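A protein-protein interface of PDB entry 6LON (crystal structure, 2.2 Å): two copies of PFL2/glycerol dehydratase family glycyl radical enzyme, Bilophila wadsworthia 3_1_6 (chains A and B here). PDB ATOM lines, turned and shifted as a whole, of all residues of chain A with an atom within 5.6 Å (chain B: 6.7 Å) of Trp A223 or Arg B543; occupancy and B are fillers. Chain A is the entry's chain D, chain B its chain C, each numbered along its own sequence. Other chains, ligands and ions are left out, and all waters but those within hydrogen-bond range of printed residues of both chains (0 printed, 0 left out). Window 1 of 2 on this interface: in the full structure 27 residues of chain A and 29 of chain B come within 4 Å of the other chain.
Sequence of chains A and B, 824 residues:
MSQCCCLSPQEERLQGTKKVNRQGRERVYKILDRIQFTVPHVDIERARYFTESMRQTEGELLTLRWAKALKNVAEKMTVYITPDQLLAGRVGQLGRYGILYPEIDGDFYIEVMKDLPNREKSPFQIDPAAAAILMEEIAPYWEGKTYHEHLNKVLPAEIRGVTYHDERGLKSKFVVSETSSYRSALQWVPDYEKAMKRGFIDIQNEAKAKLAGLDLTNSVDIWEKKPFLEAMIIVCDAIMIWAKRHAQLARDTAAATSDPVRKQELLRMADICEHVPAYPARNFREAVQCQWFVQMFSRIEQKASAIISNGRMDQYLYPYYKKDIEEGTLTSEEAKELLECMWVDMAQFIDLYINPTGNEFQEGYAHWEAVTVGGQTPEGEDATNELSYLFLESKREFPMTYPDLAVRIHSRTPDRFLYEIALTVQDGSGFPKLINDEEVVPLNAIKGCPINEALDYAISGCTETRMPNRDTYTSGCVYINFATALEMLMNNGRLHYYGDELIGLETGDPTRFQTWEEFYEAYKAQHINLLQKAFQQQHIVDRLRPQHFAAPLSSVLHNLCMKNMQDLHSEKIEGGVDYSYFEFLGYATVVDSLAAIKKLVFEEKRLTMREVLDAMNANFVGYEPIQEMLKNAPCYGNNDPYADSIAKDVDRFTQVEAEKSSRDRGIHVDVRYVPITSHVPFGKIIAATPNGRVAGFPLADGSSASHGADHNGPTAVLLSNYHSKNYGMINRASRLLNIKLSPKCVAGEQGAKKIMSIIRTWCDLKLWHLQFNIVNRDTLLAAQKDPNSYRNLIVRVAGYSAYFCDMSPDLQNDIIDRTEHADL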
ATOM      1  N   GLY A  59     -21.829  12.660  32.512  1.00  0.00           N
ATOM      2  CA  GLY A  59     -20.647  12.817  31.705  1.00  0.00           C
ATOM      3  C   GLY A  59     -19.649  11.697  31.866  1.00  0.00           C
ATOM      4  O   GLY A  59     -18.856  11.456  30.945  1.00  0.00           O
ATOM      5  N   VAL A 220      -3.548   6.147  27.312  1.00  0.00           N
ATOM      6  CA  VAL A 220      -4.912   5.666  27.093  1.00  0.00           C
ATOM      7  C   VAL A 220      -5.533   4.903  28.279  1.00  0.00           C
ATOM      8  O   VAL A 220      -6.739   5.026  28.512  1.00  0.00           O
ATOM      9  CB  VAL A 220      -4.972   4.793  25.815  1.00  0.00           C
ATOM     10  CG1 VAL A 220      -4.765   5.642  24.571  1.00  0.00           C
ATOM     11  CG2 VAL A 220      -3.961   3.638  25.884  1.00  0.00           C
ATOM     12  N   ASP A 221      -4.734   4.135  29.040  1.00  0.00           N
ATOM     13  CA  ASP A 221      -5.313   3.188  29.994  1.00  0.00           C
ATOM     14  C   ASP A 221      -6.111   3.933  31.056  1.00  0.00           C
ATOM     15  O   ASP A 221      -7.154   3.447  31.533  1.00  0.00           O
ATOM     16  CB  ASP A 221      -4.235   2.331  30.675  1.00  0.00           C
ATOM     17  CG  ASP A 221      -3.614   1.261  29.774  1.00  0.00           C
ATOM     18  OD1 ASP A 221      -3.812   1.251  28.517  1.00  0.00           O
ATOM     19  OD2 ASP A 221      -2.909   0.409  30.367  1.00  0.00           O
ATOM     20  N   ILE A 222      -5.640   5.123  31.417  1.00  0.00           N
ATOM     21  CA  ILE A 222      -6.270   5.908  32.472  1.00  0.00           C
ATOM     22  C   ILE A 222      -7.693   6.288  32.078  1.00  0.00           C
ATOM     23  O   ILE A 222      -8.560   6.448  32.936  1.00  0.00           O
ATOM     24  CB  ILE A 222      -5.385   7.134  32.806  1.00  0.00           C
ATOM     25  CG1 ILE A 222      -5.937   7.894  34.015  1.00  0.00           C
ATOM     26  CG2 ILE A 222      -5.255   8.095  31.626  1.00  0.00           C
ATOM     27  CD1 ILE A 222      -4.991   9.002  34.468  1.00  0.00           C
ATOM     28  N   TRP A 223      -7.967   6.413  30.782  1.00  0.00           N
ATOM     29  CA  TRP A 223      -9.321   6.665  30.303  1.00  0.00           C
ATOM     30  C   TRP A 223     -10.046   5.403  29.840  1.00  0.00           C
ATOM     31  O   TRP A 223     -11.221   5.218  30.173  1.00  0.00           O
ATOM     32  CB  TRP A 223      -9.277   7.691  29.168  1.00  0.00           C
ATOM     33  CG  TRP A 223     -10.617   8.136  28.733  1.00  0.00           C
ATOM     34  CD1 TRP A 223     -11.222   7.866  27.533  1.00  0.00           C
ATOM     35  CD2 TRP A 223     -11.545   8.932  29.478  1.00  0.00           C
ATOM     36  NE1 TRP A 223     -12.468   8.444  27.491  1.00  0.00           N
ATOM     37  CE2 TRP A 223     -12.686   9.117  28.659  1.00  0.00           C
ATOM     38  CE3 TRP A 223     -11.530   9.509  30.756  1.00  0.00           C
ATOM     39  CZ2 TRP A 223     -13.802   9.838  29.082  1.00  0.00           C
ATOM     40  CZ3 TRP A 223     -12.647  10.240  31.166  1.00  0.00           C
ATOM     41  CH2 TRP A 223     -13.757  10.390  30.335  1.00  0.00           C
ATOM     42  N   GLU A 224      -9.397   4.538  29.044  1.00  0.00           N
ATOM     43  CA  GLU A 224     -10.156   3.449  28.415  1.00  0.00           C
ATOM     44  C   GLU A 224     -10.511   2.317  29.384  1.00  0.00           C
ATOM     45  O   GLU A 224     -11.527   1.631  29.178  1.00  0.00           O
ATOM     46  CB  GLU A 224      -9.383   2.888  27.220  1.00  0.00           C
ATOM     47  CG  GLU A 224      -9.021   3.949  26.186  1.00  0.00           C
ATOM     48  CD  GLU A 224     -10.247   4.466  25.454  1.00  0.00           C
ATOM     49  OE1 GLU A 224     -11.139   3.633  25.239  1.00  0.00           O
ATOM     50  OE2 GLU A 224     -10.323   5.675  25.119  1.00  0.00           O
ATOM     51  N   LYS A 225      -9.706   2.111  30.428  1.00  0.00           N
ATOM     52  CA  LYS A 225      -9.779   0.930  31.286  1.00  0.00           C
ATOM     53  C   LYS A 225      -9.979   1.258  32.758  1.00  0.00           C
ATOM     54  O   LYS A 225     -10.775   0.591  33.436  1.00  0.00           O
ATOM     55  CB  LYS A 225      -8.490   0.104  31.122  1.00  0.00           C
ATOM     56  CG  LYS A 225      -8.302  -0.506  29.721  1.00  0.00           C
ATOM     57  CD  LYS A 225      -6.964  -1.228  29.622  1.00  0.00           C
ATOM     58  CE  LYS A 225      -6.844  -2.128  28.370  1.00  0.00           C
ATOM     59  NZ  LYS A 225      -7.213  -1.376  27.159  1.00  0.00           N
ATOM     60  N   LYS A 226      -9.286   2.274  33.274  1.00  0.00           N
ATOM     61  CA  LYS A 226      -9.337   2.544  34.709  1.00  0.00           C
ATOM     62  C   LYS A 226     -10.757   2.821  35.170  1.00  0.00           C
ATOM     63  O   LYS A 226     -11.193   2.226  36.174  1.00  0.00           O
ATOM     64  CB  LYS A 226      -8.390   3.705  35.037  1.00  0.00           C
ATOM     65  CG  LYS A 226      -8.436   4.115  36.487  1.00  0.00           C
ATOM     66  CD  LYS A 226      -7.189   4.895  36.903  1.00  0.00           C
ATOM     67  CE  LYS A 226      -7.368   5.603  38.273  1.00  0.00           C
ATOM     68  NZ  LYS A 226      -7.894   7.022  38.084  1.00  0.00           N
ATOM     69  N   PRO A 227     -11.530   3.662  34.487  1.00  0.00           N
ATOM     70  CA  PRO A 227     -12.893   3.950  34.964  1.00  0.00           C
ATOM     71  C   PRO A 227     -13.756   2.703  35.071  1.00  0.00           C
ATOM     72  O   PRO A 227     -14.503   2.562  36.049  1.00  0.00           O
ATOM     73  CB  PRO A 227     -13.432   4.957  33.922  1.00  0.00           C
ATOM     74  CG  PRO A 227     -12.200   5.578  33.304  1.00  0.00           C
ATOM     75  CD  PRO A 227     -11.183   4.428  33.279  1.00  0.00           C
ATOM     76  N   HIS B 150     -18.224  19.326  30.496  1.00  0.00           N
ATOM     77  CA  HIS B 150     -17.995  17.893  30.373  1.00  0.00           C
ATOM     78  C   HIS B 150     -16.531  17.553  30.648  1.00  0.00           C
ATOM     79  O   HIS B 150     -16.224  16.683  31.472  1.00  0.00           O
ATOM     80  CB  HIS B 150     -18.428  17.431  28.982  1.00  0.00           C
ATOM     81  CG  HIS B 150     -18.591  15.953  28.865  1.00  0.00           C
ATOM     82  ND1 HIS B 150     -19.090  15.343  27.735  1.00  0.00           N
ATOM     83  CD2 HIS B 150     -18.304  14.960  29.731  1.00  0.00           C
ATOM     84  CE1 HIS B 150     -19.125  14.041  27.920  1.00  0.00           C
ATOM     85  NE2 HIS B 150     -18.663  13.783  29.127  1.00  0.00           N
ATOM     86  N   VAL B 154     -15.100  15.177  33.959  1.00  0.00           N
ATOM     87  CA  VAL B 154     -14.621  13.799  33.853  1.00  0.00           C
ATOM     88  C   VAL B 154     -13.125  13.671  33.965  1.00  0.00           C
ATOM     89  O   VAL B 154     -12.624  12.544  34.012  1.00  0.00           O
ATOM     90  CB  VAL B 154     -15.046  13.139  32.525  1.00  0.00           C
ATOM     91  CG1 VAL B 154     -16.572  13.089  32.433  1.00  0.00           C
ATOM     92  CG2 VAL B 154     -14.407  13.880  31.343  1.00  0.00           C
ATOM     93  N   LEU B 155     -12.391  14.763  33.975  1.00  0.00           N
ATOM     94  CA  LEU B 155     -10.943  14.657  33.984  1.00  0.00           C
ATOM     95  C   LEU B 155     -10.461  13.841  35.186  1.00  0.00           C
ATOM     96  O   LEU B 155     -10.850  14.131  36.323  1.00  0.00           O
ATOM     97  CB  LEU B 155     -10.359  16.058  34.001  1.00  0.00           C
ATOM     98  CG  LEU B 155      -8.984  16.240  33.396  1.00  0.00           C
ATOM     99  CD1 LEU B 155      -8.965  15.840  31.945  1.00  0.00           C
ATOM    100  CD2 LEU B 155      -8.558  17.700  33.585  1.00  0.00           C
ATOM    101  N   PRO B 156      -9.650  12.802  34.982  1.00  0.00           N
ATOM    102  CA  PRO B 156      -9.148  12.030  36.127  1.00  0.00           C
ATOM    103  C   PRO B 156      -8.433  12.925  37.113  1.00  0.00           C
ATOM    104  O   PRO B 156      -7.783  13.905  36.741  1.00  0.00           O
ATOM    105  CB  PRO B 156      -8.169  11.027  35.497  1.00  0.00           C
ATOM    106  CG  PRO B 156      -8.556  10.947  34.053  1.00  0.00           C
ATOM    107  CD  PRO B 156      -9.188  12.256  33.693  1.00  0.00           C
ATOM    108  N   SER B 475      -8.933  18.339  16.786  1.00  0.00           N
ATOM    109  CA  SER B 475      -8.968  18.624  18.225  1.00  0.00           C
ATOM    110  C   SER B 475      -7.905  19.643  18.604  1.00  0.00           C
ATOM    111  O   SER B 475      -6.727  19.476  18.288  1.00  0.00           O
ATOM    112  CB  SER B 475      -8.768  17.347  19.032  1.00  0.00           C
ATOM    113  OG  SER B 475      -9.867  16.463  18.869  1.00  0.00           O
ATOM    114  N   GLN B 536      -2.308  12.076  27.946  1.00  0.00           N
ATOM    115  CA  GLN B 536      -3.538  11.576  28.551  1.00  0.00           C
ATOM    116  C   GLN B 536      -4.644  12.610  28.456  1.00  0.00           C
ATOM    117  O   GLN B 536      -5.808  12.272  28.192  1.00  0.00           O
ATOM    118  CB  GLN B 536      -3.286  11.198  30.016  1.00  0.00           C
ATOM    119  CG  GLN B 536      -2.393   9.982  30.179  1.00  0.00           C
ATOM    120  CD  GLN B 536      -1.862   9.848  31.584  1.00  0.00           C
ATOM    121  OE1 GLN B 536      -2.013  10.756  32.401  1.00  0.00           O
ATOM    122  NE2 GLN B 536      -1.232   8.712  31.875  1.00  0.00           N
ATOM    123  N   GLN B 538      -4.886  14.939  26.169  1.00  0.00           N
ATOM    124  CA  GLN B 538      -5.322  15.099  24.789  1.00  0.00           C
ATOM    125  C   GLN B 538      -6.188  13.936  24.336  1.00  0.00           C
ATOM    126  O   GLN B 538      -7.151  14.139  23.588  1.00  0.00           O
ATOM    127  CB  GLN B 538      -4.129  15.252  23.846  1.00  0.00           C
ATOM    128  CG  GLN B 538      -4.559  15.736  22.501  1.00  0.00           C
ATOM    129  CD  GLN B 538      -5.233  17.073  22.608  1.00  0.00           C
ATOM    130  OE1 GLN B 538      -4.817  17.924  23.410  1.00  0.00           O
ATOM    131  NE2 GLN B 538      -6.302  17.267  21.819  1.00  0.00           N
ATOM    132  N   HIS B 539      -5.864  12.711  24.768  1.00  0.00           N
ATOM    133  CA  HIS B 539      -6.664  11.558  24.371  1.00  0.00           C
ATOM    134  C   HIS B 539      -8.113  11.698  24.852  1.00  0.00           C
ATOM    135  O   HIS B 539      -9.064  11.339  24.136  1.00  0.00           O
ATOM    136  CB  HIS B 539      -6.056  10.264  24.914  1.00  0.00           C
ATOM    137  CG  HIS B 539      -6.879   9.066  24.586  1.00  0.00           C
ATOM    138  ND1 HIS B 539      -7.126   8.678  23.283  1.00  0.00           N
ATOM    139  CD2 HIS B 539      -7.590   8.226  25.377  1.00  0.00           C
ATOM    140  CE1 HIS B 539      -7.937   7.633  23.292  1.00  0.00           C
ATOM    141  NE2 HIS B 539      -8.233   7.336  24.551  1.00  0.00           N
ATOM    142  N   ILE B 540      -8.299  12.209  26.068  1.00  0.00           N
ATOM    143  CA  ILE B 540      -9.646  12.385  26.599  1.00  0.00           C
ATOM    144  C   ILE B 540     -10.383  13.415  25.785  1.00  0.00           C
ATOM    145  O   ILE B 540     -11.542  13.220  25.419  1.00  0.00           O
ATOM    146  CB  ILE B 540      -9.585  12.774  28.085  1.00  0.00           C
ATOM    147  CG1 ILE B 540      -9.056  11.602  28.887  1.00  0.00           C
ATOM    148  CG2 ILE B 540     -10.938  13.242  28.577  1.00  0.00           C
ATOM    149  CD1 ILE B 540      -8.389  11.994  30.185  1.00  0.00           C
ATOM    150  N   VAL B 541      -9.713  14.520  25.484  1.00  0.00           N
ATOM    151  CA  VAL B 541     -10.260  15.554  24.613  1.00  0.00           C
ATOM    152  C   VAL B 541     -10.687  14.952  23.283  1.00  0.00           C
ATOM    153  O   VAL B 541     -11.747  15.286  22.742  1.00  0.00           O
ATOM    154  CB  VAL B 541      -9.216  16.680  24.434  1.00  0.00           C
ATOM    155  CG1 VAL B 541      -9.578  17.607  23.285  1.00  0.00           C
ATOM    156  CG2 VAL B 541      -9.076  17.469  25.740  1.00  0.00           C
ATOM    157  N   ASP B 542      -9.864  14.058  22.731  1.00  0.00           N
ATOM    158  CA  ASP B 542     -10.212  13.422  21.468  1.00  0.00           C
ATOM    159  C   ASP B 542     -11.466  12.573  21.603  1.00  0.00           C
ATOM    160  O   ASP B 542     -12.238  12.466  20.652  1.00  0.00           O
ATOM    161  CB  ASP B 542      -9.062  12.570  20.977  1.00  0.00           C
ATOM    162  CG  ASP B 542      -7.857  13.389  20.588  1.00  0.00           C
ATOM    163  OD1 ASP B 542      -7.987  14.616  20.378  1.00  0.00           O
ATOM    164  OD2 ASP B 542      -6.790  12.780  20.474  1.00  0.00           O
ATOM    165  N   ARG B 543     -11.679  11.964  22.771  1.00  0.00           N
ATOM    166  CA  ARG B 543     -12.874  11.173  23.006  1.00  0.00           C
ATOM    167  C   ARG B 543     -14.121  12.021  23.252  1.00  0.00           C
ATOM    168  O   ARG B 543     -15.211  11.634  22.838  1.00  0.00           O
ATOM    169  CB  ARG B 543     -12.645  10.255  24.199  1.00  0.00           C
ATOM    170  CG  ARG B 543     -11.621   9.225  23.942  1.00  0.00           C
ATOM    171  CD  ARG B 543     -12.312   8.125  23.202  1.00  0.00           C
ATOM    172  NE  ARG B 543     -11.441   7.071  22.806  1.00  0.00           N
ATOM    173  CZ  ARG B 543     -11.883   5.956  22.257  1.00  0.00           C
ATOM    174  NH1 ARG B 543     -13.189   5.811  22.082  1.00  0.00           N
ATOM    175  NH2 ARG B 543     -11.026   5.005  21.890  1.00  0.00           N
ATOM    176  N   LEU B 544     -13.984  13.176  23.898  1.00  0.00           N
ATOM    177  CA  LEU B 544     -15.151  13.990  24.246  1.00  0.00           C
ATOM    178  C   LEU B 544     -15.597  14.901  23.104  1.00  0.00           C
ATOM    179  O   LEU B 544     -16.804  15.086  22.914  1.00  0.00           O
ATOM    180  CB  LEU B 544     -14.847  14.835  25.484  1.00  0.00           C
ATOM    181  CG  LEU B 544     -14.430  14.089  26.741  1.00  0.00           C
ATOM    182  CD1 LEU B 544     -14.243  15.046  27.917  1.00  0.00           C
ATOM    183  CD2 LEU B 544     -15.451  13.075  27.084  1.00  0.00           C
ATOM    184  N   ARG B 545     -14.661  15.470  22.320  1.00  0.00           N
ATOM    185  CA  ARG B 545     -15.062  16.460  21.323  1.00  0.00           C
ATOM    186  C   ARG B 545     -16.133  15.962  20.370  1.00  0.00           C
ATOM    187  O   ARG B 545     -17.049  16.746  20.071  1.00  0.00           O
ATOM    188  CB  ARG B 545     -13.848  16.996  20.547  1.00  0.00           C
ATOM    189  CG  ARG B 545     -13.024  18.073  21.307  1.00  0.00           C
ATOM    190  CD  ARG B 545     -11.954  18.754  20.400  1.00  0.00           C
ATOM    191  NE  ARG B 545     -12.624  19.345  19.257  1.00  0.00           N
ATOM    192  CZ  ARG B 545     -12.650  18.813  18.044  1.00  0.00           C
ATOM    193  NH1 ARG B 545     -11.981  17.692  17.764  1.00  0.00           N
ATOM    194  NH2 ARG B 545     -13.343  19.425  17.104  1.00  0.00           N
ATOM    195  N   PRO B 546     -16.108  14.715  19.879  1.00  0.00           N
ATOM    196  CA  PRO B 546     -17.168  14.267  18.949  1.00  0.00           C
ATOM    197  C   PRO B 546     -18.565  14.258  19.567  1.00  0.00           C
ATOM    198  O   PRO B 546     -19.549  14.297  18.833  1.00  0.00           O
ATOM    199  CB  PRO B 546     -16.728  12.849  18.551  1.00  0.00           C
ATOM    200  CG  PRO B 546     -15.272  12.771  18.903  1.00  0.00           C
ATOM    201  CD  PRO B 546     -15.043  13.711  20.054  1.00  0.00           C
ATOM    202  N   GLN B 547     -18.675  14.208  20.883  1.00  0.00           N
ATOM    203  CA  GLN B 547     -19.959  14.303  21.563  1.00  0.00           C
ATOM    204  C   GLN B 547     -20.509  15.727  21.581  1.00  0.00           C
ATOM    205  O   GLN B 547     -21.676  15.911  21.923  1.00  0.00           O
ATOM    206  CB  GLN B 547     -19.797  13.769  22.998  1.00  0.00           C
ATOM    207  CG  GLN B 547     -19.327  12.300  23.032  1.00  0.00           C
ATOM    208  CD  GLN B 547     -19.015  11.791  24.437  1.00  0.00           C
ATOM    209  OE1 GLN B 547     -17.939  11.252  24.699  1.00  0.00           O
ATOM    210  NE2 GLN B 547     -19.946  11.969  25.331  1.00  0.00           N
ATOM    211  N   GLU B 571     -13.959  10.698  15.238  1.00  0.00           N
ATOM    212  CA  GLU B 571     -12.609  10.360  15.687  1.00  0.00           C
ATOM    213  C   GLU B 571     -11.789   9.720  14.587  1.00  0.00           C
ATOM    214  O   GLU B 571     -10.599  10.021  14.442  1.00  0.00           O
ATOM    215  CB  GLU B 571     -12.672   9.391  16.859  1.00  0.00           C
ATOM    216  CG  GLU B 571     -12.260   9.881  18.188  1.00  0.00           C
ATOM    217  CD  GLU B 571     -12.467   8.808  19.270  1.00  0.00           C
ATOM    218  OE1 GLU B 571     -11.467   8.177  19.645  1.00  0.00           O
ATOM    219  OE2 GLU B 571     -13.619   8.589  19.721  1.00  0.00           O
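Among the printed residues, merely in contact across the chains: Gly A59 with Val B154, Val A220 with His B539, Ile A222 with Pro B156, Ile A222 with Gln B536, Trp A223 with Val B154, Trp A223 with Ile B540 and Trp A223 with Arg B543.
The backbone carbonyl oxygen (O) of Arg B543 sits close to the side-chain amide oxygen (OE1) of Gln B547 (3.3 Å).
The side-chain carboxylate of Glu B571 is in salt-bridge range of the guanidinium group of Arg B543, 3.3 Å away.
No position is printed for both chains.
NE2 of His B150 is in hydrogen-bond range of O of Gly A59 (3.0 Å).
NE2 of His B539 is in hydrogen-bond range of OE2 of Glu A224.
NE of Arg B543 lies within salt-bridge range of OE2 of Glu A224 (2.9 Å).
Printed residues of chain B within 4 Å of Ile A222: Pro B156 (3.9 Å) and Gln B536 (3.7 Å).
Printed residues of chain A within 4 Å of Ile B540: Trp A223.
Arg B543 touches just these residues of chain A: Trp A223 (3.7 Å) and Glu A224 (2.9 Å).
The nearest printed residue of chain B that does not touch Val A220 is Gln B536 (4.9 Å).
Of the 9 printed residues of chain A, 5 touch a printed residue of chain B.
Among the printed residues, 10 pairs touch across the chains.
Among the printed residues, Asp or Glu carboxylates within 4 Å of a Lys or Arg side-chain nitrogen of the other chain: Glu A224 with Arg B543 (2.9 Å).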
